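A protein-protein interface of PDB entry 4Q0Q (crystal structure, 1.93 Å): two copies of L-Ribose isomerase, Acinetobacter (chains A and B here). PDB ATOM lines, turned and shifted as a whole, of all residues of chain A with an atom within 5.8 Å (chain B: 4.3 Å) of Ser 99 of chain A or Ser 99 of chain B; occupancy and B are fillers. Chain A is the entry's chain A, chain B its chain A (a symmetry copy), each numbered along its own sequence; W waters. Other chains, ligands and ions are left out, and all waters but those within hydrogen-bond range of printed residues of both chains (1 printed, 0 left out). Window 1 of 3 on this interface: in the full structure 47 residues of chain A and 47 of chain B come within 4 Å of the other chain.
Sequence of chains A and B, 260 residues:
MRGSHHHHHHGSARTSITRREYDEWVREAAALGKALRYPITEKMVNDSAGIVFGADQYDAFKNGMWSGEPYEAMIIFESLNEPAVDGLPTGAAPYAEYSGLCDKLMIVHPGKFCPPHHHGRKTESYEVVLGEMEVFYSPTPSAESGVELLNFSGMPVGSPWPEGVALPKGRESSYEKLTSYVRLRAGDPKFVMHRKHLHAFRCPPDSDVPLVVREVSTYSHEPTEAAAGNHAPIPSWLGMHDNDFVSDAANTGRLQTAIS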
ATOM      1  N   GLU A  82      25.233  15.140  -2.093  1.00  0.00           N
ATOM      2  CA  GLU A  82      24.186  15.999  -1.574  1.00  0.00           C
ATOM      3  C   GLU A  82      24.518  16.583  -0.200  1.00  0.00           C
ATOM      4  O   GLU A  82      24.781  15.847   0.752  1.00  0.00           O
ATOM      5  CB  GLU A  82      22.888  15.183  -1.504  1.00  0.00           C
ATOM      6  CG  GLU A  82      21.772  15.808  -0.679  1.00  0.00           C
ATOM      7  CD  GLU A  82      21.335  17.155  -1.209  1.00  0.00           C
ATOM      8  OE1 GLU A  82      21.160  17.282  -2.436  1.00  0.00           O
ATOM      9  OE2 GLU A  82      21.156  18.084  -0.398  1.00  0.00           O
ATOM     10  N   PRO A  83      24.499  17.922  -0.082  1.00  0.00           N
ATOM     11  CA  PRO A  83      24.793  18.640   1.162  1.00  0.00           C
ATOM     12  C   PRO A  83      23.817  18.300   2.287  1.00  0.00           C
ATOM     13  O   PRO A  83      24.196  18.265   3.460  1.00  0.00           O
ATOM     14  CB  PRO A  83      24.695  20.113   0.747  1.00  0.00           C
ATOM     15  CG  PRO A  83      25.065  20.084  -0.715  1.00  0.00           C
ATOM     16  CD  PRO A  83      24.302  18.869  -1.196  1.00  0.00           C
ATOM     17  N   ALA A  84      22.565  18.041   1.922  1.00  0.00           N
ATOM     18  CA  ALA A  84      21.527  17.719   2.899  1.00  0.00           C
ATOM     19  C   ALA A  84      21.387  18.852   3.925  1.00  0.00           C
ATOM     20  O   ALA A  84      21.156  18.620   5.115  1.00  0.00           O
ATOM     21  CB  ALA A  84      21.851  16.409   3.602  1.00  0.00           C
ATOM     22  N   TYR A  95      27.868  22.631  11.650  1.00  0.00           N
ATOM     23  CA  TYR A  95      28.106  21.192  11.702  1.00  0.00           C
ATOM     24  C   TYR A  95      27.606  20.424  10.478  1.00  0.00           C
ATOM     25  O   TYR A  95      27.802  19.211  10.374  1.00  0.00           O
ATOM     26  CB  TYR A  95      27.468  20.615  12.965  1.00  0.00           C
ATOM     27  CG  TYR A  95      27.910  21.326  14.222  1.00  0.00           C
ATOM     28  CD1 TYR A  95      29.262  21.405  14.561  1.00  0.00           C
ATOM     29  CD2 TYR A  95      26.981  21.940  15.063  1.00  0.00           C
ATOM     30  CE1 TYR A  95      29.681  22.078  15.705  1.00  0.00           C
ATOM     31  CE2 TYR A  95      27.388  22.617  16.213  1.00  0.00           C
ATOM     32  CZ  TYR A  95      28.737  22.682  16.526  1.00  0.00           C
ATOM     33  OH  TYR A  95      29.146  23.351  17.656  1.00  0.00           O
ATOM     34  N   ALA A  96      26.980  21.131   9.545  1.00  0.00           N
ATOM     35  CA  ALA A  96      26.449  20.496   8.344  1.00  0.00           C
ATOM     36  C   ALA A  96      27.536  19.819   7.506  1.00  0.00           C
ATOM     37  O   ALA A  96      27.292  18.793   6.872  1.00  0.00           O
ATOM     38  CB  ALA A  96      25.696  21.530   7.498  1.00  0.00           C
ATOM     39  N   GLU A  97      28.735  20.389   7.516  1.00  0.00           N
ATOM     40  CA  GLU A  97      29.842  19.858   6.740  1.00  0.00           C
ATOM     41  C   GLU A  97      30.260  18.437   7.123  1.00  0.00           C
ATOM     42  O   GLU A  97      31.041  17.808   6.409  1.00  0.00           O
ATOM     43  CB  GLU A  97      31.039  20.807   6.841  1.00  0.00           C
ATOM     44  CG  GLU A  97      31.544  21.031   8.252  1.00  0.00           C
ATOM     45  CD  GLU A  97      32.382  22.288   8.363  1.00  0.00           C
ATOM     46  OE1 GLU A  97      31.821  23.387   8.183  1.00  0.00           O
ATOM     47  OE2 GLU A  97      33.597  22.182   8.615  1.00  0.00           O
ATOM     48  N   TYR A  98      29.741  17.940   8.243  1.00  0.00           N
ATOM     49  CA  TYR A  98      30.052  16.592   8.716  1.00  0.00           C
ATOM     50  C   TYR A  98      28.984  15.612   8.240  1.00  0.00           C
ATOM     51  O   TYR A  98      29.139  14.397   8.374  1.00  0.00           O
ATOM     52  CB  TYR A  98      30.098  16.565  10.245  1.00  0.00           C
ATOM     53  CG  TYR A  98      31.272  17.303  10.835  1.00  0.00           C
ATOM     54  CD1 TYR A  98      32.504  16.670  11.003  1.00  0.00           C
ATOM     55  CD2 TYR A  98      31.161  18.647  11.198  1.00  0.00           C
ATOM     56  CE1 TYR A  98      33.602  17.360  11.521  1.00  0.00           C
ATOM     57  CE2 TYR A  98      32.251  19.344  11.710  1.00  0.00           C
ATOM     58  CZ  TYR A  98      33.467  18.696  11.869  1.00  0.00           C
ATOM     59  OH  TYR A  98      34.548  19.389  12.362  1.00  0.00           O
ATOM     60  N   SER A  99      27.901  16.153   7.691  1.00  0.00           N
ATOM     61  CA  SER A  99      26.801  15.337   7.214  1.00  0.00           C
ATOM     62  C   SER A  99      26.731  15.317   5.685  1.00  0.00           C
ATOM     63  O   SER A  99      27.758  15.408   5.006  1.00  0.00           O
ATOM     64  CB  SER A  99      25.488  15.853   7.810  1.00  0.00           C
ATOM     65  OG  SER A  99      24.417  14.970   7.531  1.00  0.00           O
ATOM     66  N   GLY A 100      25.525  15.204   5.141  1.00  0.00           N
ATOM     67  CA  GLY A 100      25.386  15.152   3.697  1.00  0.00           C
ATOM     68  C   GLY A 100      25.448  13.708   3.226  1.00  0.00           C
ATOM     69  O   GLY A 100      25.717  12.809   4.023  1.00  0.00           O
ATOM     70  N   LEU A 101      25.228  13.487   1.934  1.00  0.00           N
ATOM     71  CA  LEU A 101      25.217  12.143   1.366  1.00  0.00           C
ATOM     72  C   LEU A 101      26.020  12.057   0.074  1.00  0.00           C
ATOM     73  O   LEU A 101      25.772  12.814  -0.868  1.00  0.00           O
ATOM     74  CB  LEU A 101      23.770  11.717   1.087  1.00  0.00           C
ATOM     75  CG  LEU A 101      22.836  11.612   2.304  1.00  0.00           C
ATOM     76  CD1 LEU A 101      21.388  11.433   1.848  1.00  0.00           C
ATOM     77  CD2 LEU A 101      23.280  10.453   3.186  1.00  0.00           C
ATOM     78  N   ARG A 121      36.097  15.549   8.251  1.00  0.00           N
ATOM     79  CA  ARG A 121      34.638  15.573   8.355  1.00  0.00           C
ATOM     80  C   ARG A 121      33.906  14.358   7.785  1.00  0.00           C
ATOM     81  O   ARG A 121      32.884  13.925   8.327  1.00  0.00           O
ATOM     82  CB  ARG A 121      34.114  16.832   7.661  1.00  0.00           C
ATOM     83  CG  ARG A 121      34.900  18.092   7.999  1.00  0.00           C
ATOM     84  CD  ARG A 121      34.573  19.216   7.029  1.00  0.00           C
ATOM     85  NE  ARG A 121      35.308  20.446   7.322  1.00  0.00           N
ATOM     86  CZ  ARG A 121      36.625  20.591   7.198  1.00  0.00           C
ATOM     87  NH1 ARG A 121      37.380  19.581   6.780  1.00  0.00           N
ATOM     88  NH2 ARG A 121      37.188  21.757   7.485  1.00  0.00           N
ATOM     89  N   ARG A 195      35.520   9.051  10.126  1.00  0.00           N
ATOM     90  CA  ARG A 195      36.284  10.244   9.811  1.00  0.00           C
ATOM     91  C   ARG A 195      37.467  10.298  10.780  1.00  0.00           C
ATOM     92  O   ARG A 195      37.413   9.732  11.872  1.00  0.00           O
ATOM     93  CB  ARG A 195      35.404  11.486   9.987  1.00  0.00           C
ATOM     94  CG  ARG A 195      34.803  11.616  11.386  1.00  0.00           C
ATOM     95  CD  ARG A 195      34.000  12.895  11.532  1.00  0.00           C
ATOM     96  NE  ARG A 195      32.782  12.898  10.729  1.00  0.00           N
ATOM     97  CZ  ARG A 195      31.608  12.441  11.149  1.00  0.00           C
ATOM     98  NH1 ARG A 195      31.489  11.940  12.370  1.00  0.00           N
ATOM     99  NH2 ARG A 195      30.548  12.500  10.352  1.00  0.00           N
ATOM    100  N   THR A 218      29.400  10.476   3.949  1.00  0.00           N
ATOM    101  CA  THR A 218      28.880  11.815   4.170  1.00  0.00           C
ATOM    102  C   THR A 218      29.458  12.679   3.043  1.00  0.00           C
ATOM    103  O   THR A 218      30.244  12.192   2.229  1.00  0.00           O
ATOM    104  CB  THR A 218      29.269  12.381   5.577  1.00  0.00           C
ATOM    105  OG1 THR A 218      30.692  12.384   5.742  1.00  0.00           O
ATOM    106  CG2 THR A 218      28.631  11.553   6.680  1.00  0.00           C
ATOM    107  N   TYR A 219      29.070  13.948   3.001  1.00  0.00           N
ATOM    108  CA  TYR A 219      29.493  14.868   1.950  1.00  0.00           C
ATOM    109  C   TYR A 219      30.989  14.926   1.657  1.00  0.00           C
ATOM    110  O   TYR A 219      31.817  14.951   2.561  1.00  0.00           O
ATOM    111  CB  TYR A 219      28.988  16.275   2.269  1.00  0.00           C
ATOM    112  CG  TYR A 219      29.018  17.206   1.087  1.00  0.00           C
ATOM    113  CD1 TYR A 219      28.015  17.167   0.119  1.00  0.00           C
ATOM    114  CD2 TYR A 219      30.044  18.142   0.938  1.00  0.00           C
ATOM    115  CE1 TYR A 219      28.027  18.039  -0.970  1.00  0.00           C
ATOM    116  CE2 TYR A 219      30.066  19.017  -0.144  1.00  0.00           C
ATOM    117  CZ  TYR A 219      29.053  18.963  -1.092  1.00  0.00           C
ATOM    118  OH  TYR A 219      29.051  19.846  -2.146  1.00  0.00           O
ATOM    119  N   HIS A 221      33.941  17.098   0.356  1.00  0.00           N
ATOM    120  CA  HIS A 221      34.418  18.456   0.084  1.00  0.00           C
ATOM    121  C   HIS A 221      35.692  18.349  -0.753  1.00  0.00           C
ATOM    122  O   HIS A 221      36.788  18.254  -0.203  1.00  0.00           O
ATOM    123  CB  HIS A 221      34.735  19.178   1.399  1.00  0.00           C
ATOM    124  CG  HIS A 221      33.579  19.247   2.349  1.00  0.00           C
ATOM    125  ND1 HIS A 221      32.568  20.175   2.230  1.00  0.00           N
ATOM    126  CD2 HIS A 221      33.263  18.486   3.422  1.00  0.00           C
ATOM    127  CE1 HIS A 221      31.678  19.981   3.185  1.00  0.00           C
ATOM    128  NE2 HIS A 221      32.075  18.961   3.923  1.00  0.00           N
ATOM    129  N   TRP A 237      31.904  26.236   3.254  1.00  0.00           N
ATOM    130  CA  TRP A 237      32.085  25.114   2.337  1.00  0.00           C
ATOM    131  C   TRP A 237      32.868  25.451   1.073  1.00  0.00           C
ATOM    132  O   TRP A 237      33.668  24.644   0.599  1.00  0.00           O
ATOM    133  CB  TRP A 237      30.722  24.553   1.942  1.00  0.00           C
ATOM    134  CG  TRP A 237      30.000  23.877   3.064  1.00  0.00           C
ATOM    135  CD1 TRP A 237      29.940  24.279   4.370  1.00  0.00           C
ATOM    136  CD2 TRP A 237      29.187  22.705   2.967  1.00  0.00           C
ATOM    137  NE1 TRP A 237      29.138  23.427   5.090  1.00  0.00           N
ATOM    138  CE2 TRP A 237      28.662  22.452   4.252  1.00  0.00           C
ATOM    139  CE3 TRP A 237      28.848  21.844   1.915  1.00  0.00           C
ATOM    140  CZ2 TRP A 237      27.813  21.374   4.516  1.00  0.00           C
ATOM    141  CZ3 TRP A 237      28.004  20.774   2.176  1.00  0.00           C
ATOM    142  CH2 TRP A 237      27.497  20.549   3.469  1.00  0.00           C
ATOM    143  N   TYR B  95      22.992  17.968  16.901  1.00  0.00           N
ATOM    144  CA  TYR B  95      22.670  17.951  15.478  1.00  0.00           C
ATOM    145  C   TYR B  95      23.051  16.656  14.759  1.00  0.00           C
ATOM    146  O   TYR B  95      22.775  16.494  13.568  1.00  0.00           O
ATOM    147  CB  TYR B  95      23.343  19.137  14.788  1.00  0.00           C
ATOM    148  CG  TYR B  95      23.019  20.458  15.444  1.00  0.00           C
ATOM    149  CD1 TYR B  95      21.696  20.883  15.581  1.00  0.00           C
ATOM    150  CD2 TYR B  95      24.030  21.275  15.951  1.00  0.00           C
ATOM    151  CE1 TYR B  95      21.386  22.088  16.205  1.00  0.00           C
ATOM    152  CE2 TYR B  95      23.733  22.485  16.578  1.00  0.00           C
ATOM    153  CZ  TYR B  95      22.410  22.883  16.702  1.00  0.00           C
ATOM    154  OH  TYR B  95      22.109  24.074  17.322  1.00  0.00           O
ATOM    155  N   ALA B  96      23.664  15.730  15.485  1.00  0.00           N
ATOM    156  CA  ALA B  96      24.085  14.463  14.896  1.00  0.00           C
ATOM    157  C   ALA B  96      22.911  13.655  14.335  1.00  0.00           C
ATOM    158  O   ALA B  96      23.055  12.949  13.338  1.00  0.00           O
ATOM    159  CB  ALA B  96      24.849  13.634  15.935  1.00  0.00           C
ATOM    160  N   GLU B  97      21.752  13.772  14.972  1.00  0.00           N
ATOM    161  CA  GLU B  97      20.572  13.036  14.555  1.00  0.00           C
ATOM    162  C   GLU B  97      20.090  13.360  13.139  1.00  0.00           C
ATOM    163  O   GLU B  97      19.233  12.661  12.602  1.00  0.00           O
ATOM    164  CB  GLU B  97      19.443  13.265  15.563  1.00  0.00           C
ATOM    165  CG  GLU B  97      19.035  14.715  15.729  1.00  0.00           C
ATOM    166  CD  GLU B  97      18.284  14.949  17.022  1.00  0.00           C
ATOM    167  OE1 GLU B  97      18.899  14.800  18.097  1.00  0.00           O
ATOM    168  OE2 GLU B  97      17.080  15.269  16.971  1.00  0.00           O
ATOM    169  N   TYR B  98      20.641  14.415  12.545  1.00  0.00           N
ATOM    170  CA  TYR B  98      20.276  14.828  11.191  1.00  0.00           C
ATOM    171  C   TYR B  98      21.253  14.231  10.181  1.00  0.00           C
ATOM    172  O   TYR B  98      21.032  14.304   8.972  1.00  0.00           O
ATOM    173  CB  TYR B  98      20.317  16.352  11.072  1.00  0.00           C
ATOM    174  CG  TYR B  98      19.227  17.055  11.839  1.00  0.00           C
ATOM    175  CD1 TYR B  98      17.970  17.262  11.269  1.00  0.00           C
ATOM    176  CD2 TYR B  98      19.441  17.488  13.149  1.00  0.00           C
ATOM    177  CE1 TYR B  98      16.948  17.885  11.988  1.00  0.00           C
ATOM    178  CE2 TYR B  98      18.427  18.106  13.875  1.00  0.00           C
ATOM    179  CZ  TYR B  98      17.185  18.301  13.290  1.00  0.00           C
ATOM    180  OH  TYR B  98      16.178  18.898  14.013  1.00  0.00           O
ATOM    181  N   SER B  99      22.334  13.649  10.692  1.00  0.00           N
ATOM    182  CA  SER B  99      23.353  13.059   9.845  1.00  0.00           C
ATOM    183  C   SER B  99      23.332  11.530   9.916  1.00  0.00           C
ATOM    184  O   SER B  99      22.275  10.922  10.107  1.00  0.00           O
ATOM    185  CB  SER B  99      24.727  13.603  10.247  1.00  0.00           C
ATOM    186  OG  SER B  99      25.724  13.207   9.322  1.00  0.00           O
ATOM    187  N   GLY B 100      24.496  10.908   9.767  1.00  0.00           N
ATOM    188  CA  GLY B 100      24.548   9.457   9.796  1.00  0.00           C
ATOM    189  C   GLY B 100      24.371   8.908   8.390  1.00  0.00           C
ATOM    190  O   GLY B 100      24.094   9.666   7.460  1.00  0.00           O
ATOM    191  N   THR B 218      20.276   9.683   5.353  1.00  0.00           N
ATOM    192  CA  THR B 218      20.889   9.949   6.643  1.00  0.00           C
ATOM    193  C   THR B 218      20.301   8.912   7.607  1.00  0.00           C
ATOM    194  O   THR B 218      19.441   8.120   7.217  1.00  0.00           O
ATOM    195  CB  THR B 218      20.617  11.407   7.143  1.00  0.00           C
ATOM    196  OG1 THR B 218      19.209  11.659   7.217  1.00  0.00           O
ATOM    197  CG2 THR B 218      21.266  12.419   6.213  1.00  0.00           C
ATOM    198  N   TYR B 219      20.764   8.920   8.852  1.00  0.00           N
ATOM    199  CA  TYR B 219      20.338   7.952   9.857  1.00  0.00           C
ATOM    200  C   TYR B 219      18.834   7.754  10.020  1.00  0.00           C
ATOM    201  O   TYR B 219      18.062   8.708  10.037  1.00  0.00           O
ATOM    202  CB  TYR B 219      20.945   8.321  11.211  1.00  0.00           C
ATOM    203  CG  TYR B 219      20.904   7.199  12.213  1.00  0.00           C
ATOM    204  CD1 TYR B 219      21.846   6.170  12.176  1.00  0.00           C
ATOM    205  CD2 TYR B 219      19.930   7.167  13.214  1.00  0.00           C
ATOM    206  CE1 TYR B 219      21.825   5.137  13.113  1.00  0.00           C
ATOM    207  CE2 TYR B 219      19.900   6.142  14.154  1.00  0.00           C
ATOM    208  CZ  TYR B 219      20.851   5.131  14.100  1.00  0.00           C
ATOM    209  OH  TYR B 219      20.847   4.132  15.045  1.00  0.00           O
HETATM  210  O   HOH W   1      27.593  13.296  11.456  1.00  0.00           O
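The side-chain hydroxyl of Ser 99 of chain A is in hydrogen-bond range of the side-chain hydroxyl of Ser 99 of chain B.
The backbone carbonyl oxygen (O) of Glu 82 of chain A lies within hydrogen-bond range of the backbone NH (N) of Leu 101 of chain A (2.7 Å).
NH2 of Arg 195 of chain A is in hydrogen-bond range of O of Tyr 98 of chain A.
The backbone carbonyl oxygen (O) of Ser 99 of chain A is in hydrogen-bond range of the backbone NH (N) of Tyr 219 of chain A (2.8 Å).
The backbone carbonyl oxygen (O) of Ser 99 of chain B is in hydrogen-bond range of the backbone NH (N) of Tyr 219 of chain B, 2.8 Å away.
Tyr 95 of chain B touches Tyr 95 of chain A (CD2 to CD2, 3.2 Å).
Tyr 98 of chain A touches Ser 99 of chain B.
OG of Ser 99 of chain A touches O of Tyr 98 of chain B, 3.7 Å away.
Leu 101 of chain A touches Thr 218 of chain B (CD2 to N, 3.8 Å).
Ser 99 of chain A touches just these residues of chain B: Tyr 98 (3.7 Å) and Ser 99 (2.8 Å).
Of chain A, only Tyr 98 and Ser 99 come within 4 Å of Ser 99 of chain B.
Of the printed residues of chain B, Tyr 98 of chain A touches Ser 99.
Of the printed residues of chain A, Thr 218 of chain B touches Leu 101 (3.8 Å).
Of the printed residues of chain A, Tyr 95 of chain B touches Tyr 95.
Of the printed residues of chain B, Leu 101 of chain A touches Thr 218 (3.8 Å).
Thr 218 of chain A touches none of the printed residues of chain B.
Ala 84 of chain A touches none of the printed residues of chain B.
The nearest printed residue of chain B that does not touch Ser 99 of chain A is Thr 218 of chain B (4.3 Å).
The nearest printed residue of chain A that does not touch Tyr 95 of chain B is Ser 99 of chain A (6.4 Å).
Of the 8 printed residues of chain B, 4 touch a printed residue of chain A.
Among the printed residues, 5 pairs touch across the chains.
Tyr 95 of chain B touches its own counterpart, Tyr 95 of chain A.
Tyr 98 of chain A touches Ser 99 of chain B, and with the chains exchanged Ser 99 of chain A touches Tyr 98 of chain B.
Ser 99 of chain A touches its own counterpart, Ser 99 of chain B.
Of the 5 pairs that touch across the chains among the printed residues, 4 have their exchanged pair printed and touching as well.
Water W1 bridges the side-chain hydroxyl of Ser 99 of chain B and the guanidinium group of Arg 195 of chain A.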
